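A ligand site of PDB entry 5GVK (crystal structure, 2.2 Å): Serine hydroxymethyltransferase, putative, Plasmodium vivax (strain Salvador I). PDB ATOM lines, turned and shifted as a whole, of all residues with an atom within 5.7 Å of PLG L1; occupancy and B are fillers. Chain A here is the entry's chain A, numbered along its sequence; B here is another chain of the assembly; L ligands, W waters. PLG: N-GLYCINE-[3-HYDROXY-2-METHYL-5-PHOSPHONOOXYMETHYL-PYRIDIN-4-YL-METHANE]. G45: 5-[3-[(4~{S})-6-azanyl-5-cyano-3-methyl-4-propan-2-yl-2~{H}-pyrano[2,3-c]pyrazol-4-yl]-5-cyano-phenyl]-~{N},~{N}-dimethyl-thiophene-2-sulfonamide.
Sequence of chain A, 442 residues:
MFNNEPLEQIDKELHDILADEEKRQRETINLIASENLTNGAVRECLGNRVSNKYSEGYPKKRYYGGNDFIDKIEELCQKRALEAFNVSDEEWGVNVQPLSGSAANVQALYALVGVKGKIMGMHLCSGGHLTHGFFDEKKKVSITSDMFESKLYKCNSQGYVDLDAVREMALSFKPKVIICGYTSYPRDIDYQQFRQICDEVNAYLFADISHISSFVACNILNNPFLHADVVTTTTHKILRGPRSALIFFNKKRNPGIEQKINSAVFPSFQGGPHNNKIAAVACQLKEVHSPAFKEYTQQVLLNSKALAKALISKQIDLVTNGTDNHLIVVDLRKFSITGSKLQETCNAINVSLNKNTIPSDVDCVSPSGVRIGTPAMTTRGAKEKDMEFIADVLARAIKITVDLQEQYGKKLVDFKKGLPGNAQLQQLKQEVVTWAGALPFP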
ATOM      1  N   ILE A  32      26.110  33.916  26.840  1.00  0.00           N
ATOM      2  CA  ILE A  32      26.634  32.611  26.390  1.00  0.00           C
ATOM      3  C   ILE A  32      25.770  32.154  25.219  1.00  0.00           C
ATOM      4  O   ILE A  32      24.559  31.974  25.361  1.00  0.00           O
ATOM      5  CB  ILE A  32      26.583  31.521  27.476  1.00  0.00           C
ATOM      6  CG1 ILE A  32      27.061  32.055  28.860  1.00  0.00           C
ATOM      7  CG2 ILE A  32      27.315  30.289  26.982  1.00  0.00           C
ATOM      8  CD1 ILE A  32      28.531  31.895  29.204  1.00  0.00           C
ATOM      9  N   SER A  34      25.461  29.421  23.578  1.00  0.00           N
ATOM     10  CA  SER A  34      24.868  28.099  23.790  1.00  0.00           C
ATOM     11  C   SER A  34      23.896  27.964  24.987  1.00  0.00           C
ATOM     12  O   SER A  34      23.463  26.850  25.298  1.00  0.00           O
ATOM     13  CB  SER A  34      25.998  27.105  23.980  1.00  0.00           C
ATOM     14  OG  SER A  34      26.843  27.577  25.028  1.00  0.00           O
ATOM     15  N   SER A 100      23.170  13.718  25.303  1.00  0.00           N
ATOM     16  CA  SER A 100      23.662  15.064  25.060  1.00  0.00           C
ATOM     17  C   SER A 100      24.264  15.159  23.667  1.00  0.00           C
ATOM     18  O   SER A 100      24.399  14.143  22.957  1.00  0.00           O
ATOM     19  CB  SER A 100      24.716  15.461  26.113  1.00  0.00           C
ATOM     20  OG  SER A 100      24.461  16.772  26.608  1.00  0.00           O
ATOM     21  N   GLY A 101      24.660  16.377  23.289  1.00  0.00           N
ATOM     22  CA  GLY A 101      25.241  16.634  22.011  1.00  0.00           C
ATOM     23  C   GLY A 101      26.444  15.819  21.658  1.00  0.00           C
ATOM     24  O   GLY A 101      26.531  15.289  20.529  1.00  0.00           O
ATOM     25  N   SER A 102      27.376  15.696  22.598  1.00  0.00           N
ATOM     26  CA  SER A 102      28.644  15.021  22.337  1.00  0.00           C
ATOM     27  C   SER A 102      28.410  13.525  22.163  1.00  0.00           C
ATOM     28  O   SER A 102      28.996  12.903  21.265  1.00  0.00           O
ATOM     29  CB  SER A 102      29.674  15.287  23.460  1.00  0.00           C
ATOM     30  OG  SER A 102      29.855  16.662  23.685  1.00  0.00           O
ATOM     31  N   ALA A 103      27.509  12.968  22.985  1.00  0.00           N
ATOM     32  CA  ALA A 103      27.029  11.580  22.855  1.00  0.00           C
ATOM     33  C   ALA A 103      26.413  11.311  21.473  1.00  0.00           C
ATOM     34  O   ALA A 103      26.876  10.434  20.763  1.00  0.00           O
ATOM     35  CB  ALA A 103      26.055  11.228  23.975  1.00  0.00           C
ATOM     36  N   ASN A 105      26.698  12.934  18.679  1.00  0.00           N
ATOM     37  CA  ASN A 105      27.677  13.015  17.614  1.00  0.00           C
ATOM     38  C   ASN A 105      28.548  11.761  17.516  1.00  0.00           C
ATOM     39  O   ASN A 105      28.829  11.305  16.412  1.00  0.00           O
ATOM     40  CB  ASN A 105      28.560  14.257  17.709  1.00  0.00           C
ATOM     41  CG  ASN A 105      27.858  15.525  17.254  1.00  0.00           C
ATOM     42  OD1 ASN A 105      26.698  15.503  16.891  1.00  0.00           O
ATOM     43  ND2 ASN A 105      28.568  16.637  17.289  1.00  0.00           N
ATOM     44  N   HIS A 129      33.416  22.005  16.530  1.00  0.00           N
ATOM     45  CA  HIS A 129      33.244  21.395  17.846  1.00  0.00           C
ATOM     46  C   HIS A 129      34.310  20.376  18.115  1.00  0.00           C
ATOM     47  O   HIS A 129      34.927  19.858  17.190  1.00  0.00           O
ATOM     48  CB  HIS A 129      31.869  20.750  18.018  1.00  0.00           C
ATOM     49  CG  HIS A 129      31.543  20.416  19.444  1.00  0.00           C
ATOM     50  ND1 HIS A 129      31.526  19.126  19.931  1.00  0.00           N
ATOM     51  CD2 HIS A 129      31.273  21.223  20.503  1.00  0.00           C
ATOM     52  CE1 HIS A 129      31.244  19.148  21.223  1.00  0.00           C
ATOM     53  NE2 HIS A 129      31.079  20.413  21.596  1.00  0.00           N
ATOM     54  N   THR A 131      33.787  17.346  19.086  1.00  0.00           N
ATOM     55  CA  THR A 131      33.320  16.063  18.558  1.00  0.00           C
ATOM     56  C   THR A 131      33.368  15.978  17.024  1.00  0.00           C
ATOM     57  O   THR A 131      32.894  15.001  16.417  1.00  0.00           O
ATOM     58  CB  THR A 131      31.917  15.714  19.079  1.00  0.00           C
ATOM     59  OG1 THR A 131      30.988  16.719  18.662  1.00  0.00           O
ATOM     60  CG2 THR A 131      31.921  15.628  20.616  1.00  0.00           C
ATOM     61  N   HIS A 132      33.970  16.994  16.405  1.00  0.00           N
ATOM     62  CA  HIS A 132      34.155  17.017  14.961  1.00  0.00           C
ATOM     63  C   HIS A 132      35.586  16.594  14.604  1.00  0.00           C
ATOM     64  O   HIS A 132      36.135  17.026  13.606  1.00  0.00           O
ATOM     65  CB  HIS A 132      33.763  18.384  14.361  1.00  0.00           C
ATOM     66  CG  HIS A 132      32.357  18.805  14.657  1.00  0.00           C
ATOM     67  ND1 HIS A 132      31.873  20.055  14.336  1.00  0.00           N
ATOM     68  CD2 HIS A 132      31.335  18.162  15.276  1.00  0.00           C
ATOM     69  CE1 HIS A 132      30.604  20.153  14.699  1.00  0.00           C
ATOM     70  NE2 HIS A 132      30.257  19.020  15.285  1.00  0.00           N
ATOM     71  N   GLY A 181      28.268  22.533  10.125  1.00  0.00           N
ATOM     72  CA  GLY A 181      27.430  23.010  11.272  1.00  0.00           C
ATOM     73  C   GLY A 181      28.323  23.065  12.523  1.00  0.00           C
ATOM     74  O   GLY A 181      29.063  22.106  12.810  1.00  0.00           O
ATOM     75  N   TYR A 182      28.307  24.184  13.252  1.00  0.00           N
ATOM     76  CA  TYR A 182      29.476  24.520  14.071  1.00  0.00           C
ATOM     77  C   TYR A 182      29.171  25.077  15.450  1.00  0.00           C
ATOM     78  O   TYR A 182      27.999  25.333  15.770  1.00  0.00           O
ATOM     79  CB  TYR A 182      30.415  25.452  13.297  1.00  0.00           C
ATOM     80  CG  TYR A 182      30.741  24.969  11.895  1.00  0.00           C
ATOM     81  CD1 TYR A 182      31.528  23.826  11.672  1.00  0.00           C
ATOM     82  CD2 TYR A 182      30.263  25.660  10.774  1.00  0.00           C
ATOM     83  CE1 TYR A 182      31.827  23.390  10.378  1.00  0.00           C
ATOM     84  CE2 TYR A 182      30.559  25.248   9.482  1.00  0.00           C
ATOM     85  CZ  TYR A 182      31.341  24.110   9.291  1.00  0.00           C
ATOM     86  OH  TYR A 182      31.620  23.708   8.010  1.00  0.00           O
ATOM     87  N   THR A 183      30.205  25.259  16.252  1.00  0.00           N
ATOM     88  CA  THR A 183      29.991  25.774  17.615  1.00  0.00           C
ATOM     89  C   THR A 183      30.172  27.284  17.741  1.00  0.00           C
ATOM     90  O   THR A 183      29.410  27.941  18.467  1.00  0.00           O
ATOM     91  CB  THR A 183      30.703  24.990  18.743  1.00  0.00           C
ATOM     92  OG1 THR A 183      31.531  25.862  19.521  1.00  0.00           O
ATOM     93  CG2 THR A 183      31.555  23.978  18.231  1.00  0.00           C
ATOM     94  N   ASP A 208      25.620  19.235  11.938  1.00  0.00           N
ATOM     95  CA  ASP A 208      25.379  19.409  13.358  1.00  0.00           C
ATOM     96  C   ASP A 208      24.885  20.815  13.484  1.00  0.00           C
ATOM     97  O   ASP A 208      25.642  21.751  13.292  1.00  0.00           O
ATOM     98  CB  ASP A 208      26.686  19.196  14.127  1.00  0.00           C
ATOM     99  CG  ASP A 208      26.553  19.422  15.623  1.00  0.00           C
ATOM    100  OD1 ASP A 208      25.527  19.912  16.134  1.00  0.00           O
ATOM    101  OD2 ASP A 208      27.510  19.098  16.296  1.00  0.00           O
ATOM    102  N   SER A 210      23.173  22.186  16.213  1.00  0.00           N
ATOM    103  CA  SER A 210      22.871  22.474  17.623  1.00  0.00           C
ATOM    104  C   SER A 210      22.756  23.959  17.916  1.00  0.00           C
ATOM    105  O   SER A 210      21.810  24.380  18.592  1.00  0.00           O
ATOM    106  CB  SER A 210      23.907  21.843  18.559  1.00  0.00           C
ATOM    107  OG  SER A 210      24.176  20.487  18.243  1.00  0.00           O
ATOM    108  N   HIS A 211      23.705  24.738  17.401  1.00  0.00           N
ATOM    109  CA  HIS A 211      23.685  26.188  17.598  1.00  0.00           C
ATOM    110  C   HIS A 211      22.605  26.953  16.850  1.00  0.00           C
ATOM    111  O   HIS A 211      22.189  28.036  17.278  1.00  0.00           O
ATOM    112  CB  HIS A 211      25.064  26.802  17.361  1.00  0.00           C
ATOM    113  CG  HIS A 211      25.865  26.895  18.618  1.00  0.00           C
ATOM    114  ND1 HIS A 211      25.787  27.977  19.475  1.00  0.00           N
ATOM    115  CD2 HIS A 211      26.726  26.028  19.193  1.00  0.00           C
ATOM    116  CE1 HIS A 211      26.576  27.768  20.516  1.00  0.00           C
ATOM    117  NE2 HIS A 211      27.160  26.589  20.366  1.00  0.00           N
ATOM    118  N   THR A 234      21.522  19.357  19.637  1.00  0.00           N
ATOM    119  CA  THR A 234      21.172  19.388  21.053  1.00  0.00           C
ATOM    120  C   THR A 234      19.817  20.056  21.203  1.00  0.00           C
ATOM    121  O   THR A 234      19.388  20.766  20.295  1.00  0.00           O
ATOM    122  CB  THR A 234      22.229  20.193  21.817  1.00  0.00           C
ATOM    123  OG1 THR A 234      22.319  21.505  21.250  1.00  0.00           O
ATOM    124  CG2 THR A 234      23.579  19.535  21.686  1.00  0.00           C
ATOM    125  N   HIS A 236      19.111  22.016  24.134  1.00  0.00           N
ATOM    126  CA  HIS A 236      19.251  23.011  25.220  1.00  0.00           C
ATOM    127  C   HIS A 236      19.691  24.417  24.809  1.00  0.00           C
ATOM    128  O   HIS A 236      19.659  25.355  25.627  1.00  0.00           O
ATOM    129  CB  HIS A 236      20.182  22.492  26.332  1.00  0.00           C
ATOM    130  CG  HIS A 236      21.383  21.749  25.839  1.00  0.00           C
ATOM    131  ND1 HIS A 236      21.315  20.440  25.384  1.00  0.00           N
ATOM    132  CD2 HIS A 236      22.677  22.122  25.720  1.00  0.00           C
ATOM    133  CE1 HIS A 236      22.523  20.042  25.025  1.00  0.00           C
ATOM    134  NE2 HIS A 236      23.360  21.041  25.208  1.00  0.00           N
ATOM    135  N   LYS A 237      20.110  24.584  23.562  1.00  0.00           N
ATOM    136  CA  LYS A 237      20.628  25.867  23.151  1.00  0.00           C
ATOM    137  C   LYS A 237      19.501  26.775  22.632  1.00  0.00           C
ATOM    138  O   LYS A 237      18.564  27.106  23.365  1.00  0.00           O
ATOM    139  CB  LYS A 237      21.769  25.735  22.157  1.00  0.00           C
ATOM    140  CG  LYS A 237      22.940  24.908  22.655  1.00  0.00           C
ATOM    141  CD  LYS A 237      24.032  24.906  21.598  1.00  0.00           C
ATOM    142  CE  LYS A 237      25.161  23.952  21.970  1.00  0.00           C
ATOM    143  NZ  LYS A 237      24.701  22.729  22.663  1.00  0.00           N
ATOM    144  N   ARG A 243      18.492  19.558  28.472  1.00  0.00           N
ATOM    145  CA  ARG A 243      19.801  19.146  28.018  1.00  0.00           C
ATOM    146  C   ARG A 243      19.680  17.725  27.488  1.00  0.00           C
ATOM    147  O   ARG A 243      19.557  16.778  28.256  1.00  0.00           O
ATOM    148  CB  ARG A 243      20.832  19.209  29.146  1.00  0.00           C
ATOM    149  CG  ARG A 243      20.950  20.579  29.807  1.00  0.00           C
ATOM    150  CD  ARG A 243      22.240  20.660  30.636  1.00  0.00           C
ATOM    151  NE  ARG A 243      23.407  20.806  29.766  1.00  0.00           N
ATOM    152  CZ  ARG A 243      23.852  21.972  29.309  1.00  0.00           C
ATOM    153  NH1 ARG A 243      23.238  23.121  29.666  1.00  0.00           N
ATOM    154  NH2 ARG A 243      24.902  21.994  28.495  1.00  0.00           N
ATOM    155  N   SER A 244      19.688  17.612  26.163  1.00  0.00           N
ATOM    156  CA  SER A 244      19.531  16.331  25.474  1.00  0.00           C
ATOM    157  C   SER A 244      19.934  16.510  24.026  1.00  0.00           C
ATOM    158  O   SER A 244      20.295  17.621  23.644  1.00  0.00           O
ATOM    159  CB  SER A 244      18.074  15.861  25.538  1.00  0.00           C
ATOM    160  OG  SER A 244      18.045  14.493  25.220  1.00  0.00           O
ATOM    161  N   ASN A 354      31.811  33.685  27.076  1.00  0.00           N
ATOM    162  CA  ASN A 354      32.988  32.838  27.073  1.00  0.00           C
ATOM    163  C   ASN A 354      34.076  33.320  26.150  1.00  0.00           C
ATOM    164  O   ASN A 354      33.811  33.959  25.111  1.00  0.00           O
ATOM    165  CB  ASN A 354      32.639  31.354  26.765  1.00  0.00           C
ATOM    166  CG  ASN A 354      32.217  31.124  25.311  1.00  0.00           C
ATOM    167  OD1 ASN A 354      31.044  31.288  24.973  1.00  0.00           O
ATOM    168  ND2 ASN A 354      33.179  30.743  24.461  1.00  0.00           N
ATOM    169  N   ARG A 371      33.132  34.984  22.652  1.00  0.00           N
ATOM    170  CA  ARG A 371      31.940  34.730  21.871  1.00  0.00           C
ATOM    171  C   ARG A 371      30.705  35.233  22.657  1.00  0.00           C
ATOM    172  O   ARG A 371      30.640  35.096  23.877  1.00  0.00           O
ATOM    173  CB  ARG A 371      31.841  33.247  21.538  1.00  0.00           C
ATOM    174  CG  ARG A 371      30.724  32.849  20.589  1.00  0.00           C
ATOM    175  CD  ARG A 371      30.428  31.354  20.627  1.00  0.00           C
ATOM    176  NE  ARG A 371      29.964  30.917  21.950  1.00  0.00           N
ATOM    177  CZ  ARG A 371      29.732  29.663  22.295  1.00  0.00           C
ATOM    178  NH1 ARG A 371      29.911  28.672  21.421  1.00  0.00           N
ATOM    179  NH2 ARG A 371      29.320  29.387  23.530  1.00  0.00           N
ATOM    180  N   TYR B  54      25.937  26.195  31.180  1.00  0.00           N
ATOM    181  CA  TYR B  54      27.054  25.513  30.505  1.00  0.00           C
ATOM    182  C   TYR B  54      28.300  25.683  31.352  1.00  0.00           C
ATOM    183  O   TYR B  54      28.696  26.798  31.700  1.00  0.00           O
ATOM    184  CB  TYR B  54      27.326  26.071  29.088  1.00  0.00           C
ATOM    185  CG  TYR B  54      27.137  25.021  28.002  1.00  0.00           C
ATOM    186  CD1 TYR B  54      28.062  23.954  27.849  1.00  0.00           C
ATOM    187  CD2 TYR B  54      26.020  25.054  27.175  1.00  0.00           C
ATOM    188  CE1 TYR B  54      27.858  22.984  26.878  1.00  0.00           C
ATOM    189  CE2 TYR B  54      25.805  24.084  26.196  1.00  0.00           C
ATOM    190  CZ  TYR B  54      26.714  23.063  26.061  1.00  0.00           C
ATOM    191  OH  TYR B  54      26.471  22.128  25.118  1.00  0.00           O
ATOM    192  N   GLU B  56      31.418  23.383  30.997  1.00  0.00           N
ATOM    193  CA  GLU B  56      32.502  22.482  30.562  1.00  0.00           C
ATOM    194  C   GLU B  56      33.784  22.695  31.328  1.00  0.00           C
ATOM    195  O   GLU B  56      34.170  23.835  31.602  1.00  0.00           O
ATOM    196  CB  GLU B  56      32.802  22.616  29.080  1.00  0.00           C
ATOM    197  CG  GLU B  56      31.638  22.182  28.200  1.00  0.00           C
ATOM    198  CD  GLU B  56      31.976  22.260  26.742  1.00  0.00           C
ATOM    199  OE1 GLU B  56      32.738  21.422  26.257  1.00  0.00           O
ATOM    200  OE2 GLU B  56      31.495  23.188  26.099  1.00  0.00           O
ATOM    201  N   TYR B  64      33.471  28.861  30.783  1.00  0.00           N
ATOM    202  CA  TYR B  64      32.403  29.863  30.764  1.00  0.00           C
ATOM    203  C   TYR B  64      32.444  30.680  32.045  1.00  0.00           C
ATOM    204  O   TYR B  64      32.902  30.186  33.090  1.00  0.00           O
ATOM    205  CB  TYR B  64      31.000  29.212  30.569  1.00  0.00           C
ATOM    206  CG  TYR B  64      30.933  28.282  29.374  1.00  0.00           C
ATOM    207  CD1 TYR B  64      31.303  26.935  29.496  1.00  0.00           C
ATOM    208  CD2 TYR B  64      30.530  28.753  28.115  1.00  0.00           C
ATOM    209  CE1 TYR B  64      31.282  26.081  28.414  1.00  0.00           C
ATOM    210  CE2 TYR B  64      30.509  27.908  27.007  1.00  0.00           C
ATOM    211  CZ  TYR B  64      30.873  26.567  27.161  1.00  0.00           C
ATOM    212  OH  TYR B  64      30.864  25.708  26.100  1.00  0.00           O
ATOM    213  N   GLN B 270      32.403  13.675  26.747  1.00  0.00           N
ATOM    214  CA  GLN B 270      31.297  14.593  27.014  1.00  0.00           C
ATOM    215  C   GLN B 270      31.672  16.047  26.742  1.00  0.00           C
ATOM    216  O   GLN B 270      32.836  16.344  26.507  1.00  0.00           O
ATOM    217  CB  GLN B 270      30.704  14.423  28.423  1.00  0.00           C
ATOM    218  CG  GLN B 270      30.494  12.971  28.866  1.00  0.00           C
ATOM    219  CD  GLN B 270      29.568  12.779  30.064  1.00  0.00           C
ATOM    220  OE1 GLN B 270      28.945  11.723  30.197  1.00  0.00           O
ATOM    221  NE2 GLN B 270      29.480  13.788  30.953  1.00  0.00           N
ATOM    222  N   GLY B 271      30.644  16.910  26.716  1.00  0.00           N
ATOM    223  CA  GLY B 271      30.732  18.326  26.636  1.00  0.00           C
ATOM    224  C   GLY B 271      30.191  18.890  27.945  1.00  0.00           C
ATOM    225  O   GLY B 271      30.705  18.570  29.006  1.00  0.00           O
ATOM    226  N   GLY B 272      29.153  19.701  27.875  1.00  0.00           N
ATOM    227  CA  GLY B 272      28.613  20.339  29.076  1.00  0.00           C
ATOM    228  C   GLY B 272      28.017  19.383  30.090  1.00  0.00           C
ATOM    229  O   GLY B 272      27.186  18.561  29.733  1.00  0.00           O
ATOM    230  N   HIS B 274      25.576  17.901  33.080  1.00  0.00           N
ATOM    231  CA  HIS B 274      24.189  18.125  33.452  1.00  0.00           C
ATOM    232  C   HIS B 274      24.067  18.423  34.938  1.00  0.00           C
ATOM    233  O   HIS B 274      23.959  17.533  35.790  1.00  0.00           O
ATOM    234  CB  HIS B 274      23.282  16.960  32.999  1.00  0.00           C
ATOM    235  CG  HIS B 274      23.212  16.784  31.519  1.00  0.00           C
ATOM    236  ND1 HIS B 274      22.280  15.961  30.910  1.00  0.00           N
ATOM    237  CD2 HIS B 274      23.938  17.319  30.504  1.00  0.00           C
ATOM    238  CE1 HIS B 274      22.458  15.982  29.602  1.00  0.00           C
ATOM    239  NE2 HIS B 274      23.457  16.806  29.333  1.00  0.00           N
HETATM  240  N1  PLG L   1      27.786  20.266  18.793  1.00  0.00           N
HETATM  241  C2  PLG L   1      27.983  21.590  18.726  1.00  0.00           C
HETATM  242  C2A PLG L   1      28.011  22.261  17.363  1.00  0.00           C
HETATM  243  C3  PLG L   1      28.142  22.352  20.002  1.00  0.00           C
HETATM  244  O3  PLG L   1      28.315  23.682  19.982  1.00  0.00           O
HETATM  245  C4  PLG L   1      28.069  21.622  21.311  1.00  0.00           C
HETATM  246  C4A PLG L   1      28.242  22.377  22.631  1.00  0.00           C
HETATM  247  C5  PLG L   1      27.861  20.147  21.221  1.00  0.00           C
HETATM  248  C6  PLG L   1      27.732  19.577  19.959  1.00  0.00           C
HETATM  249  C5A PLG L   1      27.806  19.181  22.401  1.00  0.00           C
HETATM  250  OP4 PLG L   1      26.752  19.411  23.335  1.00  0.00           O
HETATM  251  P   PLG L   1      26.885  18.839  24.830  1.00  0.00           P
HETATM  252  OP1 PLG L   1      27.681  17.581  24.729  1.00  0.00           O
HETATM  253  OP2 PLG L   1      27.638  19.930  25.547  1.00  0.00           O
HETATM  254  OP3 PLG L   1      25.432  18.751  25.201  1.00  0.00           O
HETATM  255  C   PLG L   1      29.064  25.704  23.358  1.00  0.00           C
HETATM  256  O   PLG L   1      28.974  26.487  24.296  1.00  0.00           O
HETATM  257  OXT PLG L   1      28.804  26.065  22.188  1.00  0.00           O
HETATM  258  CA  PLG L   1      29.520  24.271  23.661  1.00  0.00           C
HETATM  259  N   PLG L   1      29.300  23.359  22.560  1.00  0.00           N
HETATM  260  N9  G45 L   2      36.707  28.555  20.486  1.00  0.00           N
HETATM  261  C8  G45 L   2      36.090  27.622  20.811  1.00  0.00           C
HETATM  262  N7  G45 L   2      35.168  26.014  18.896  1.00  0.00           N
HETATM  263  C5  G45 L   2      34.635  24.960  22.862  1.00  0.00           C
HETATM  264  C6  G45 L   2      34.135  24.126  21.772  1.00  0.00           C
HETATM  265  C2  G45 L   2      34.952  25.771  20.194  1.00  0.00           C
HETATM  266  C4  G45 L   2      35.167  26.353  22.668  1.00  0.00           C
HETATM  267  O35 G45 L   2      41.876  20.778  26.466  1.00  0.00           O
HETATM  268  S30 G45 L   2      41.714  20.962  25.047  1.00  0.00           S
HETATM  269  O34 G45 L   2      40.960  19.832  24.634  1.00  0.00           O
HETATM  270  N31 G45 L   2      43.131  21.052  24.419  1.00  0.00           N
HETATM  271  C33 G45 L   2      43.875  22.151  25.025  1.00  0.00           C
HETATM  272  C32 G45 L   2      43.028  21.260  22.988  1.00  0.00           C
HETATM  273  C28 G45 L   2      40.642  22.194  24.792  1.00  0.00           C
HETATM  274  C27 G45 L   2      39.334  21.939  25.132  1.00  0.00           C
HETATM  275  C26 G45 L   2      38.539  23.046  24.885  1.00  0.00           C
HETATM  276  S29 G45 L   2      40.884  23.797  24.204  1.00  0.00           S
HETATM  277  C25 G45 L   2      39.199  24.142  24.374  1.00  0.00           C
HETATM  278  C21 G45 L   2      38.606  25.445  24.056  1.00  0.00           C
HETATM  279  C20 G45 L   2      39.191  26.696  24.294  1.00  0.00           C
HETATM  280  C19 G45 L   2      38.433  27.846  23.967  1.00  0.00           C
HETATM  281  C23 G45 L   2      38.921  29.008  24.153  1.00  0.00           C
HETATM  282  N24 G45 L   2      39.360  30.055  24.309  1.00  0.00           N
HETATM  283  C18 G45 L   2      37.138  27.707  23.472  1.00  0.00           C
HETATM  284  C22 G45 L   2      37.311  25.344  23.546  1.00  0.00           C
HETATM  285  C17 G45 L   2      36.547  26.461  23.266  1.00  0.00           C
HETATM  286  C14 G45 L   2      34.170  27.380  23.252  1.00  0.00           C
HETATM  287  C16 G45 L   2      34.007  27.397  24.796  1.00  0.00           C
HETATM  288  C15 G45 L   2      32.771  27.364  22.598  1.00  0.00           C
HETATM  289  C3  G45 L   2      35.414  26.593  21.166  1.00  0.00           C
HETATM  290  C10 G45 L   2      34.415  24.043  24.027  1.00  0.00           C
HETATM  291  C13 G45 L   2      34.721  24.272  25.487  1.00  0.00           C
HETATM  292  N11 G45 L   2      33.881  22.907  23.532  1.00  0.00           N
HETATM  293  N12 G45 L   2      33.721  22.920  22.139  1.00  0.00           N
HETATM  294  O1  G45 L   2      34.161  24.592  20.504  1.00  0.00           O
HETATM  295  O   HOH W   1      25.358  19.585  27.881  1.00  0.00           O
HETATM  296  O   HOH W   2      27.761  16.101  27.358  1.00  0.00           O
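The backbone NH (N) of Gly 101 is in hydrogen-bond range of an oxygen (OP3) of PLG L1 (3.1 Å). An oxygen (OXT) of PLG L1 lies within salt-bridge range of the guanidinium group (NH1) of Arg 371 (2.9 Å). An oxygen (O1) of G45 L2 lies within hydrogen-bond range of the side-chain hydroxyl (OG1) of Thr 183, 3.1 Å away. OP1 of PLG L1 sits at hydrogen-bond distance from OG of Ser 102, 2.6 Å away. A nitrogen (N1) of PLG L1 lies within hydrogen-bond range of the side-chain carboxylate of Asp 208 (2.8 Å). The side-chain hydroxyl of Ser 100 lies within hydrogen-bond range of an oxygen (OP3) of PLG L1 (2.6 Å). An oxygen (OXT) of PLG L1 lies within hydrogen-bond range of a ring nitrogen (NE2) of His 211. An oxygen (O) of PLG L1 is in hydrogen-bond range of the side-chain hydroxyl (OH) of Tyr 64 of chain B, at 2.7 Å. NE2 of His 236 lies within hydrogen-bond range of OP3 of PLG L1 (3.1 Å). An oxygen (OP2) of PLG L1 lies within hydrogen-bond range of the backbone NH of Gly 272 of chain B. An oxygen (O) of PLG L1 is in hydrogen-bond range of the side-chain hydroxyl (OG) of Ser 34 (2.5 Å). The backbone NH of Ser 102 sits at hydrogen-bond distance from an oxygen (OP1) of PLG L1, at 2.9 Å. The side-chain carboxylate (OE1) of Glu 56 of chain B lies within hydrogen-bond range of a nitrogen (N11) of G45 L2, at 3.3 Å. OH of Tyr 54 of chain B lies within hydrogen-bond range of OP2 of PLG L1 (2.5 Å).
His 129 touches PLG L1 (NE2 to C5, 3.3 Å). Tyr 182 touches PLG L1 (O to C2A, 3.5 Å). Thr 183 touches PLG L1 (CB to O3, 3.0 Å). OG of Ser 210 touches N1 of PLG L1 (3.7 Å). Thr 234 touches PLG L1 (CG2 to OP4, 3.6 Å). Lys 237 touches PLG L1 (CE to C4A, 3.5 Å). OE2 of Glu 56 of chain B touches CA of PLG L1, 3.3 Å away. Gly 271 of chain B touches PLG L1. Hydrophobic or aromatic side chains that line PLG L1: His 129, His 211, His 236, Tyr 54 of chain B and Tyr 64 of chain B. Of the 30 residues printed, 19 come within 4 Å of PLG L1.
A ring nitrogen (NE2) of His 236 is in hydrogen-bond range of the side-chain hydroxyl (OH) of Tyr 54 of chain B (3.3 Å). ND1 of His 132 lies within hydrogen-bond range of N of His 129 (3.3 Å). NH2 of Arg 371 sits at hydrogen-bond distance from OG of Ser 34 (3.4 Å). The side-chain hydroxyl (OG) of Ser 100 sits at hydrogen-bond distance from a ring nitrogen (NE2) of His 274 of chain B, at 2.9 Å. The side-chain carboxylate (OE2) of Glu 56 of chain B lies within hydrogen-bond range of the side-chain hydroxyl (OH) of Tyr 64 of chain B. The side-chain hydroxyl of Tyr 54 of chain B lies within hydrogen-bond range of the side-chain amino group of Lys 237, 3.1 Å away. The side-chain carboxylate of Asp 208 sits at hydrogen-bond distance from a ring nitrogen (NE2) of His 132, 2.9 Å away. The backbone NH of Arg 371 is in hydrogen-bond range of the backbone carbonyl oxygen of Asn 354, 2.7 Å away.
Water W1 lies within hydrogen-bond range of the guanidinium group (NH2) of Arg 243 (2.5 Å), the backbone carbonyl oxygen (O) of Gly 272 of chain B (2.8 Å), an oxygen (OP3) of PLG L1 (2.8 Å) and the side-chain hydroxyl (OG) of Ser 100 (3.2 Å). Water W2 lies within hydrogen-bond range of an oxygen (OP1) of PLG L1 (3.0 Å), the backbone NH (N) of Gly 271 of chain B (3.1 Å), the side-chain hydroxyl (OG) of Ser 100 (3.5 Å) and the backbone carbonyl oxygen (O) of Gly 272 of chain B (3.5 Å).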
